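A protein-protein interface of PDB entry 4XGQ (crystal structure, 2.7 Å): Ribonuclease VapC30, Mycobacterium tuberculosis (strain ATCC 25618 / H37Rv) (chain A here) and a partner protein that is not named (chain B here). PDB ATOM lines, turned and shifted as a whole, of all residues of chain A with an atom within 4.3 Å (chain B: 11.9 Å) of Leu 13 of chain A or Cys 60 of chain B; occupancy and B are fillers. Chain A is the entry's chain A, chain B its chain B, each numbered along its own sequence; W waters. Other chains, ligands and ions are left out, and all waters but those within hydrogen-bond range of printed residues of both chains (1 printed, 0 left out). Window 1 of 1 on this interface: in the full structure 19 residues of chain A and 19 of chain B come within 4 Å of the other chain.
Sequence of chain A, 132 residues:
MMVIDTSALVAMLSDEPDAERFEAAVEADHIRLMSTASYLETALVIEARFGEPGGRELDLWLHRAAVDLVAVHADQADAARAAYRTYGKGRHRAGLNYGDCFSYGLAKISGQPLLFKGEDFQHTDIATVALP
The guanidinium group (NH2) of Arg 59 of chain B lies within salt-bridge range of the side-chain carboxylate (OE1) of Glu 57 of chain A, 2.7 Å away.
The backbone NH (N) of Ala 61 of chain B sits at hydrogen-bond distance from the backbone carbonyl oxygen (O) of Leu 13 of chain A (3.5 Å).
The side-chain carboxylate (OD1) of Asp 15 of chain A lies within salt-bridge range of the guanidinium group (NH1) of Arg 57 of chain B (2.5 Å).
Leu 13 of chain A touches four residues of chain B.
No residue of chain B comes within 4 Å of Leu 9 of chain A.
Val 10 of chain A touches none of the printed residues of chain B.
Ala 11 of chain A touches none of the printed residues of chain B.
Met 12 of chain A touches just one residue of chain B: Arg 57.
Of chain B, only Ala 61 (3.7 Å) comes within 4 Å of Ser 14 of chain A.
Asp 15 of chain A touches just these residues of chain B: Arg 57, His 58 and Ala 61.
No residue of chain B comes within 4 Å of Ile 46 of chain A.
Phe 50 of chain A touches just these residues of chain B: Cys 60, Leu 63 and Pro 64.
Of the printed residues of chain A, Ile 56 of chain B touches Leu 13 and Glu 57.
Of the printed residues of chain A, Leu 63 of chain B touches Phe 50 and Gly 54.
Printed residues of chain A within 4 Å of Arg 59 of chain B: Glu 57.
Of the printed residues of chain A, Arg 57 of chain B touches Met 12 (3.1 Å), Leu 13 (3.7 Å) and Asp 15 (2.5 Å).
Leu 53 of chain B touches none of the printed residues of chain A.
Arg 50 of chain B touches none of the printed residues of chain A.
The nearest residue of chain B that does not touch Leu 13 of chain A is His 58 of chain B (5.8 Å).
The nearest residue of chain A that does not touch Cys 60 of chain B is Gly 54 of chain A (4.1 Å).
Hydrophobic or aromatic side chains of chain B within 4 Å of the printed part of chain A: Ile 56, His 58, Ala 61 and Leu 63.
Of the 12 printed residues of chain A, 7 touch a printed residue of chain B.
Printed residues of chain A that touch a printed residue of chain B: Met 12, Leu 13, Ser 14, Asp 15, Phe 50, Gly 54 and Glu 57.
Among the printed residues, Asp or Glu carboxylates within 4 Å of a Lys or Arg side-chain nitrogen of the other chain: Asp 15 of chain A with Arg 57 of chain B (2.5 Å) and Glu 57 of chain A with Arg 59 of chain B (2.7 Å).
Water W1 lies within hydrogen-bond range of O of Leu 53 of chain B and O of Met 12 of chain A.
Met 12 of chain A touches Arg 57 of chain B.
Leu 13 of chain A touches Ile 56 of chain B.
O of Arg 57 of chain B touches O of Leu 13 of chain A (3.7 Å).
Cys 60 of chain B touches Leu 13 of chain A.
Ala 61 of chain B touches Ser 14 of chain A.
CB of Asp 15 of chain A touches CB of Ala 61 of chain B, 3.5 Å away.
Cys 60 of chain B touches Phe 50 of chain A (O to CD1, 3.8 Å).
Leu 63 of chain B touches Phe 50 of chain A.
Pro 64 of chain B touches Phe 50 of chain A (O to CA, 3.8 Å).
Glu 57 of chain A touches Ile 56 of chain B (O to CG2, 3.7 Å).
O of Ala 54 of chain B is in hydrogen-bond range of ND1 of His 58 of chain B.
The backbone carbonyl oxygen (O) of Val 10 of chain A lies within hydrogen-bond range of the side-chain hydroxyl (OG) of Ser 14 of chain A, 2.9 Å away.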
ATOM      1  N   LEU A   9      -1.033  11.397  15.773  1.00  0.00           N
ATOM      2  CA  LEU A   9      -2.254  12.141  16.141  1.00  0.00           C
ATOM      3  C   LEU A   9      -3.032  12.627  14.945  1.00  0.00           C
ATOM      4  O   LEU A   9      -4.263  12.636  14.958  1.00  0.00           O
ATOM      5  CB  LEU A   9      -1.904  13.314  17.023  1.00  0.00           C
ATOM      6  CG  LEU A   9      -2.998  14.206  17.582  1.00  0.00           C
ATOM      7  CD1 LEU A   9      -4.157  13.436  18.192  1.00  0.00           C
ATOM      8  CD2 LEU A   9      -2.331  15.067  18.634  1.00  0.00           C
ATOM      9  N   VAL A  10      -2.318  13.012  13.898  1.00  0.00           N
ATOM     10  CA  VAL A  10      -2.963  13.430  12.648  1.00  0.00           C
ATOM     11  C   VAL A  10      -3.661  12.244  11.982  1.00  0.00           C
ATOM     12  O   VAL A  10      -4.696  12.387  11.315  1.00  0.00           O
ATOM     13  CB  VAL A  10      -1.922  14.021  11.693  1.00  0.00           C
ATOM     14  CG1 VAL A  10      -2.503  14.242  10.292  1.00  0.00           C
ATOM     15  CG2 VAL A  10      -1.354  15.322  12.275  1.00  0.00           C
ATOM     16  N   ALA A  11      -3.077  11.068  12.156  1.00  0.00           N
ATOM     17  CA  ALA A  11      -3.676   9.840  11.661  1.00  0.00           C
ATOM     18  C   ALA A  11      -4.936   9.571  12.464  1.00  0.00           C
ATOM     19  O   ALA A  11      -5.979   9.298  11.913  1.00  0.00           O
ATOM     20  CB  ALA A  11      -2.690   8.672  11.779  1.00  0.00           C
ATOM     21  N   MET A  12      -4.838   9.697  13.774  1.00  0.00           N
ATOM     22  CA  MET A  12      -5.973   9.397  14.617  1.00  0.00           C
ATOM     23  C   MET A  12      -7.126  10.391  14.446  1.00  0.00           C
ATOM     24  O   MET A  12      -8.222  10.119  14.906  1.00  0.00           O
ATOM     25  CB  MET A  12      -5.554   9.356  16.073  1.00  0.00           C
ATOM     26  CG  MET A  12      -5.157   8.002  16.542  1.00  0.00           C
ATOM     27  SD  MET A  12      -4.667   7.999  18.269  1.00  0.00           S
ATOM     28  CE  MET A  12      -3.020   8.690  18.070  1.00  0.00           C
ATOM     29  N   LEU A  13      -6.878  11.542  13.831  1.00  0.00           N
ATOM     30  CA  LEU A  13      -7.913  12.560  13.684  1.00  0.00           C
ATOM     31  C   LEU A  13      -8.451  12.571  12.278  1.00  0.00           C
ATOM     32  O   LEU A  13      -9.600  12.939  12.085  1.00  0.00           O
ATOM     33  CB  LEU A  13      -7.382  13.957  14.074  1.00  0.00           C
ATOM     34  CG  LEU A  13      -7.146  14.173  15.581  1.00  0.00           C
ATOM     35  CD1 LEU A  13      -6.268  15.370  15.865  1.00  0.00           C
ATOM     36  CD2 LEU A  13      -8.449  14.337  16.339  1.00  0.00           C
ATOM     37  N   SER A  14      -7.627  12.221  11.288  1.00  0.00           N
ATOM     38  CA  SER A  14      -8.102  12.158   9.898  1.00  0.00           C
ATOM     39  C   SER A  14      -8.808  10.842   9.568  1.00  0.00           C
ATOM     40  O   SER A  14      -9.334  10.718   8.473  1.00  0.00           O
ATOM     41  CB  SER A  14      -6.957  12.350   8.904  1.00  0.00           C
ATOM     42  OG  SER A  14      -6.252  13.543   9.144  1.00  0.00           O
ATOM     43  N   ASP A  15      -8.800   9.876  10.498  1.00  0.00           N
ATOM     44  CA  ASP A  15      -9.454   8.554  10.354  1.00  0.00           C
ATOM     45  C   ASP A  15      -8.755   7.732   9.293  1.00  0.00           C
ATOM     46  O   ASP A  15      -9.389   7.142   8.429  1.00  0.00           O
ATOM     47  CB  ASP A  15     -10.967   8.701  10.057  1.00  0.00           C
ATOM     48  CG  ASP A  15     -11.824   7.470  10.506  1.00  0.00           C
ATOM     49  OD1 ASP A  15     -11.286   6.425  10.947  1.00  0.00           O
ATOM     50  OD2 ASP A  15     -13.074   7.578  10.425  1.00  0.00           O
ATOM     51  N   ILE A  46      -3.892  19.987  10.977  1.00  0.00           N
ATOM     52  CA  ILE A  46      -5.312  19.845  11.242  1.00  0.00           C
ATOM     53  C   ILE A  46      -6.079  21.107  10.891  1.00  0.00           C
ATOM     54  O   ILE A  46      -6.988  21.057  10.078  1.00  0.00           O
ATOM     55  CB  ILE A  46      -5.574  19.476  12.710  1.00  0.00           C
ATOM     56  CG1 ILE A  46      -5.055  18.078  13.007  1.00  0.00           C
ATOM     57  CG2 ILE A  46      -7.043  19.544  13.031  1.00  0.00           C
ATOM     58  CD1 ILE A  46      -5.672  17.004  12.132  1.00  0.00           C
ATOM     59  N   PHE A  50      -9.118  21.039   8.247  1.00  0.00           N
ATOM     60  CA  PHE A  50     -10.473  21.048   8.777  1.00  0.00           C
ATOM     61  C   PHE A  50     -10.847  22.362   9.453  1.00  0.00           C
ATOM     62  O   PHE A  50     -11.838  22.423  10.199  1.00  0.00           O
ATOM     63  CB  PHE A  50     -10.612  19.928   9.805  1.00  0.00           C
ATOM     64  CG  PHE A  50     -10.298  18.575   9.258  1.00  0.00           C
ATOM     65  CD1 PHE A  50     -11.075  18.027   8.236  1.00  0.00           C
ATOM     66  CD2 PHE A  50      -9.247  17.834   9.771  1.00  0.00           C
ATOM     67  CE1 PHE A  50     -10.790  16.774   7.726  1.00  0.00           C
ATOM     68  CE2 PHE A  50      -8.957  16.578   9.265  1.00  0.00           C
ATOM     69  CZ  PHE A  50      -9.730  16.048   8.240  1.00  0.00           C
ATOM     70  N   GLY A  54     -11.504  21.819  13.451  1.00  0.00           N
ATOM     71  CA  GLY A  54     -10.590  20.681  13.593  1.00  0.00           C
ATOM     72  C   GLY A  54      -9.660  20.880  14.778  1.00  0.00           C
ATOM     73  O   GLY A  54      -9.370  19.948  15.542  1.00  0.00           O
ATOM     74  N   GLU A  57     -11.238  19.885  17.957  1.00  0.00           N
ATOM     75  CA  GLU A  57     -11.149  18.435  18.175  1.00  0.00           C
ATOM     76  C   GLU A  57      -9.760  18.016  18.631  1.00  0.00           C
ATOM     77  O   GLU A  57      -9.617  17.158  19.506  1.00  0.00           O
ATOM     78  CB  GLU A  57     -11.604  17.637  16.944  1.00  0.00           C
ATOM     79  CG  GLU A  57     -13.057  17.900  16.491  1.00  0.00           C
ATOM     80  CD  GLU A  57     -14.099  17.629  17.575  1.00  0.00           C
ATOM     81  OE1 GLU A  57     -13.849  16.779  18.452  1.00  0.00           O
ATOM     82  OE2 GLU A  57     -15.177  18.277  17.560  1.00  0.00           O
ATOM     83  N   LEU A  58      -8.737  18.651  18.070  1.00  0.00           N
ATOM     84  CA  LEU A  58      -7.354  18.441  18.539  1.00  0.00           C
ATOM     85  C   LEU A  58      -7.197  18.797  20.000  1.00  0.00           C
ATOM     86  O   LEU A  58      -6.574  18.061  20.756  1.00  0.00           O
ATOM     87  CB  LEU A  58      -6.374  19.264  17.710  1.00  0.00           C
ATOM     88  CG  LEU A  58      -4.924  19.348  18.233  1.00  0.00           C
ATOM     89  CD1 LEU A  58      -4.348  17.967  18.445  1.00  0.00           C
ATOM     90  CD2 LEU A  58      -4.057  20.129  17.246  1.00  0.00           C
ATOM     91  N   LEU B  49     -11.713   4.859  27.443  1.00  0.00           N
ATOM     92  CA  LEU B  49     -10.978   5.925  26.739  1.00  0.00           C
ATOM     93  C   LEU B  49     -10.880   5.712  25.219  1.00  0.00           C
ATOM     94  O   LEU B  49     -11.010   6.672  24.470  1.00  0.00           O
ATOM     95  CB  LEU B  49      -9.591   6.091  27.365  1.00  0.00           C
ATOM     96  CG  LEU B  49      -8.601   7.076  26.731  1.00  0.00           C
ATOM     97  CD1 LEU B  49      -9.174   8.477  26.606  1.00  0.00           C
ATOM     98  CD2 LEU B  49      -7.311   7.065  27.539  1.00  0.00           C
ATOM     99  N   ARG B  50     -10.653   4.473  24.779  1.00  0.00           N
ATOM    100  CA  ARG B  50     -10.788   4.088  23.351  1.00  0.00           C
ATOM    101  C   ARG B  50     -12.047   4.638  22.680  1.00  0.00           C
ATOM    102  O   ARG B  50     -11.993   5.104  21.542  1.00  0.00           O
ATOM    103  CB  ARG B  50     -10.874   2.573  23.203  1.00  0.00           C
ATOM    104  CG  ARG B  50      -9.580   1.883  22.849  1.00  0.00           C
ATOM    105  CD  ARG B  50      -9.765   0.359  22.793  1.00  0.00           C
ATOM    106  NE  ARG B  50     -10.192  -0.236  24.082  1.00  0.00           N
ATOM    107  CZ  ARG B  50     -11.454  -0.491  24.458  1.00  0.00           C
ATOM    108  NH1 ARG B  50     -12.480  -0.197  23.668  1.00  0.00           N
ATOM    109  NH2 ARG B  50     -11.697  -1.028  25.649  1.00  0.00           N
ATOM    110  N   ASP B  51     -13.187   4.545  23.369  1.00  0.00           N
ATOM    111  CA  ASP B  51     -14.463   4.972  22.781  1.00  0.00           C
ATOM    112  C   ASP B  51     -14.542   6.494  22.698  1.00  0.00           C
ATOM    113  O   ASP B  51     -15.144   7.039  21.772  1.00  0.00           O
ATOM    114  CB  ASP B  51     -15.677   4.405  23.561  1.00  0.00           C
ATOM    115  CG  ASP B  51     -15.753   2.868  23.542  1.00  0.00           C
ATOM    116  OD1 ASP B  51     -15.145   2.195  22.655  1.00  0.00           O
ATOM    117  OD2 ASP B  51     -16.420   2.345  24.458  1.00  0.00           O
ATOM    118  N   GLU B  52     -13.936   7.179  23.661  1.00  0.00           N
ATOM    119  CA  GLU B  52     -13.882   8.637  23.616  1.00  0.00           C
ATOM    120  C   GLU B  52     -13.011   9.165  22.462  1.00  0.00           C
ATOM    121  O   GLU B  52     -13.385  10.102  21.767  1.00  0.00           O
ATOM    122  CB  GLU B  52     -13.386   9.201  24.961  1.00  0.00           C
ATOM    123  CG  GLU B  52     -14.505   9.640  25.885  1.00  0.00           C
ATOM    124  CD  GLU B  52     -15.441  10.669  25.225  1.00  0.00           C
ATOM    125  OE1 GLU B  52     -15.053  11.293  24.192  1.00  0.00           O
ATOM    126  OE2 GLU B  52     -16.586  10.829  25.733  1.00  0.00           O
ATOM    127  N   LEU B  53     -11.861   8.553  22.255  1.00  0.00           N
ATOM    128  CA  LEU B  53     -10.974   8.984  21.195  1.00  0.00           C
ATOM    129  C   LEU B  53     -11.579   8.720  19.825  1.00  0.00           C
ATOM    130  O   LEU B  53     -11.429   9.531  18.882  1.00  0.00           O
ATOM    131  CB  LEU B  53      -9.614   8.290  21.324  1.00  0.00           C
ATOM    132  CG  LEU B  53      -8.888   8.474  22.665  1.00  0.00           C
ATOM    133  CD1 LEU B  53      -7.598   7.656  22.679  1.00  0.00           C
ATOM    134  CD2 LEU B  53      -8.613   9.947  22.926  1.00  0.00           C
ATOM    135  N   ALA B  54     -12.277   7.594  19.724  1.00  0.00           N
ATOM    136  CA  ALA B  54     -12.996   7.242  18.509  1.00  0.00           C
ATOM    137  C   ALA B  54     -14.087   8.272  18.225  1.00  0.00           C
ATOM    138  O   ALA B  54     -14.289   8.726  17.072  1.00  0.00           O
ATOM    139  CB  ALA B  54     -13.584   5.847  18.654  1.00  0.00           C
ATOM    140  N   ALA B  55     -14.768   8.669  19.287  1.00  0.00           N
ATOM    141  CA  ALA B  55     -15.820   9.662  19.154  1.00  0.00           C
ATOM    142  C   ALA B  55     -15.262  10.912  18.472  1.00  0.00           C
ATOM    143  O   ALA B  55     -15.758  11.325  17.410  1.00  0.00           O
ATOM    144  CB  ALA B  55     -16.406   9.990  20.517  1.00  0.00           C
ATOM    145  N   ILE B  56     -14.185  11.439  19.073  1.00  0.00           N
ATOM    146  CA  ILE B  56     -13.454  12.586  18.582  1.00  0.00           C
ATOM    147  C   ILE B  56     -12.933  12.361  17.172  1.00  0.00           C
ATOM    148  O   ILE B  56     -13.030  13.257  16.325  1.00  0.00           O
ATOM    149  CB  ILE B  56     -12.274  12.910  19.532  1.00  0.00           C
ATOM    150  CG1 ILE B  56     -12.816  13.413  20.889  1.00  0.00           C
ATOM    151  CG2 ILE B  56     -11.336  13.940  18.919  1.00  0.00           C
ATOM    152  CD1 ILE B  56     -11.827  13.307  22.032  1.00  0.00           C
ATOM    153  N   ARG B  57     -12.411  11.178  16.895  1.00  0.00           N
ATOM    154  CA  ARG B  57     -11.924  10.898  15.530  1.00  0.00           C
ATOM    155  C   ARG B  57     -13.021  11.041  14.465  1.00  0.00           C
ATOM    156  O   ARG B  57     -12.852  11.754  13.485  1.00  0.00           O
ATOM    157  CB  ARG B  57     -11.326   9.474  15.441  1.00  0.00           C
ATOM    158  CG  ARG B  57     -11.073   8.980  14.007  1.00  0.00           C
ATOM    159  CD  ARG B  57     -10.089   7.837  13.987  1.00  0.00           C
ATOM    160  NE  ARG B  57     -10.450   6.759  14.889  1.00  0.00           N
ATOM    161  CZ  ARG B  57     -11.146   5.688  14.541  1.00  0.00           C
ATOM    162  NH1 ARG B  57     -11.569   5.549  13.290  1.00  0.00           N
ATOM    163  NH2 ARG B  57     -11.417   4.759  15.468  1.00  0.00           N
ATOM    164  N   HIS B  58     -14.144  10.350  14.655  1.00  0.00           N
ATOM    165  CA  HIS B  58     -15.219  10.391  13.641  1.00  0.00           C
ATOM    166  C   HIS B  58     -15.756  11.820  13.404  1.00  0.00           C
ATOM    167  O   HIS B  58     -15.987  12.242  12.260  1.00  0.00           O
ATOM    168  CB  HIS B  58     -16.375   9.417  13.990  1.00  0.00           C
ATOM    169  CG  HIS B  58     -15.982   7.969  13.938  1.00  0.00           C
ATOM    170  ND1 HIS B  58     -16.104   7.121  15.026  1.00  0.00           N
ATOM    171  CD2 HIS B  58     -15.443   7.228  12.938  1.00  0.00           C
ATOM    172  CE1 HIS B  58     -15.661   5.918  14.696  1.00  0.00           C
ATOM    173  NE2 HIS B  58     -15.256   5.959  13.438  1.00  0.00           N
ATOM    174  N   ARG B  59     -15.949  12.576  14.482  1.00  0.00           N
ATOM    175  CA  ARG B  59     -16.394  13.959  14.305  1.00  0.00           C
ATOM    176  C   ARG B  59     -15.377  14.670  13.452  1.00  0.00           C
ATOM    177  O   ARG B  59     -15.729  15.209  12.415  1.00  0.00           O
ATOM    178  CB  ARG B  59     -16.526  14.682  15.627  1.00  0.00           C
ATOM    179  CG  ARG B  59     -17.860  14.520  16.302  1.00  0.00           C
ATOM    180  CD  ARG B  59     -18.185  15.736  17.174  1.00  0.00           C
ATOM    181  NE  ARG B  59     -17.115  16.032  18.119  1.00  0.00           N
ATOM    182  CZ  ARG B  59     -16.813  15.299  19.194  1.00  0.00           C
ATOM    183  NH1 ARG B  59     -17.484  14.194  19.502  1.00  0.00           N
ATOM    184  NH2 ARG B  59     -15.807  15.664  19.976  1.00  0.00           N
ATOM    185  N   CYS B  60     -14.108  14.631  13.878  1.00  0.00           N
ATOM    186  CA  CYS B  60     -13.076  15.459  13.259  1.00  0.00           C
ATOM    187  C   CYS B  60     -12.896  15.135  11.786  1.00  0.00           C
ATOM    188  O   CYS B  60     -12.793  16.031  10.943  1.00  0.00           O
ATOM    189  CB  CYS B  60     -11.749  15.311  13.988  1.00  0.00           C
ATOM    190  SG  CYS B  60     -10.532  16.541  13.484  1.00  0.00           S
ATOM    191  N   ALA B  61     -12.892  13.841  11.483  1.00  0.00           N
ATOM    192  CA  ALA B  61     -12.765  13.378  10.122  1.00  0.00           C
ATOM    193  C   ALA B  61     -14.017  13.672   9.289  1.00  0.00           C
ATOM    194  O   ALA B  61     -13.933  13.825   8.053  1.00  0.00           O
ATOM    195  CB  ALA B  61     -12.455  11.894  10.125  1.00  0.00           C
ATOM    196  N   ALA B  62     -15.163  13.776   9.961  1.00  0.00           N
ATOM    197  CA  ALA B  62     -16.421  14.119   9.286  1.00  0.00           C
ATOM    198  C   ALA B  62     -16.536  15.592   8.934  1.00  0.00           C
ATOM    199  O   ALA B  62     -17.466  15.993   8.213  1.00  0.00           O
ATOM    200  CB  ALA B  62     -17.614  13.708  10.146  1.00  0.00           C
ATOM    201  N   LEU B  63     -15.615  16.406   9.450  1.00  0.00           N
ATOM    202  CA  LEU B  63     -15.668  17.836   9.191  1.00  0.00           C
ATOM    203  C   LEU B  63     -15.374  18.138   7.725  1.00  0.00           C
ATOM    204  O   LEU B  63     -14.707  17.357   7.039  1.00  0.00           O
ATOM    205  CB  LEU B  63     -14.697  18.592  10.083  1.00  0.00           C
ATOM    206  CG  LEU B  63     -14.953  18.597  11.604  1.00  0.00           C
ATOM    207  CD1 LEU B  63     -13.764  19.208  12.360  1.00  0.00           C
ATOM    208  CD2 LEU B  63     -16.199  19.355  11.965  1.00  0.00           C
ATOM    209  N   PRO B  64     -15.884  19.276   7.234  1.00  0.00           N
ATOM    210  CA  PRO B  64     -15.565  19.620   5.867  1.00  0.00           C
ATOM    211  C   PRO B  64     -14.090  19.950   5.701  1.00  0.00           C
ATOM    212  O   PRO B  64     -13.482  20.614   6.561  1.00  0.00           O
ATOM    213  CB  PRO B  64     -16.449  20.833   5.562  1.00  0.00           C
ATOM    214  CG  PRO B  64     -17.132  21.205   6.828  1.00  0.00           C
ATOM    215  CD  PRO B  64     -16.877  20.163   7.859  1.00  0.00           C
ATOM    216  N   VAL B  65     -13.533  19.478   4.596  1.00  0.00           N
ATOM    217  CA  VAL B  65     -12.207  19.865   4.162  1.00  0.00           C
ATOM    218  C   VAL B  65     -12.246  21.289   3.619  1.00  0.00           C
ATOM    219  O   VAL B  65     -13.135  21.625   2.870  1.00  0.00           O
ATOM    220  CB  VAL B  65     -11.695  18.918   3.065  1.00  0.00           C
ATOM    221  CG1 VAL B  65     -10.389  19.434   2.490  1.00  0.00           C
ATOM    222  CG2 VAL B  65     -11.521  17.511   3.625  1.00  0.00           C
ATOM    223  N   VAL B  66     -11.283  22.122   4.024  1.00  0.00           N
ATOM    224  CA  VAL B  66     -11.173  23.501   3.541  1.00  0.00           C
ATOM    225  C   VAL B  66      -9.808  23.819   2.922  1.00  0.00           C
ATOM    226  O   VAL B  66      -9.620  24.905   2.373  1.00  0.00           O
ATOM    227  CB  VAL B  66     -11.507  24.518   4.660  1.00  0.00           C
ATOM    228  CG1 VAL B  66     -12.974  24.411   5.042  1.00  0.00           C
ATOM    229  CG2 VAL B  66     -10.637  24.335   5.890  1.00  0.00           C
ATOM    230  N   ASP B  67      -8.881  22.860   3.004  1.00  0.00           N
ATOM    231  CA  ASP B  67      -7.545  22.953   2.417  1.00  0.00           C
ATOM    232  C   ASP B  67      -6.982  21.526   2.350  1.00  0.00           C
ATOM    233  O   ASP B  67      -7.075  20.764   3.320  1.00  0.00           O
ATOM    234  CB  ASP B  67      -6.643  23.848   3.284  1.00  0.00           C
ATOM    235  CG  ASP B  67      -5.263  24.114   2.663  1.00  0.00           C
ATOM    236  OD1 ASP B  67      -5.123  24.072   1.421  1.00  0.00           O
ATOM    237  OD2 ASP B  67      -4.318  24.380   3.441  1.00  0.00           O
HETATM  238  O   HOH W   1      -8.532   9.416  18.088  1.00  0.00           O
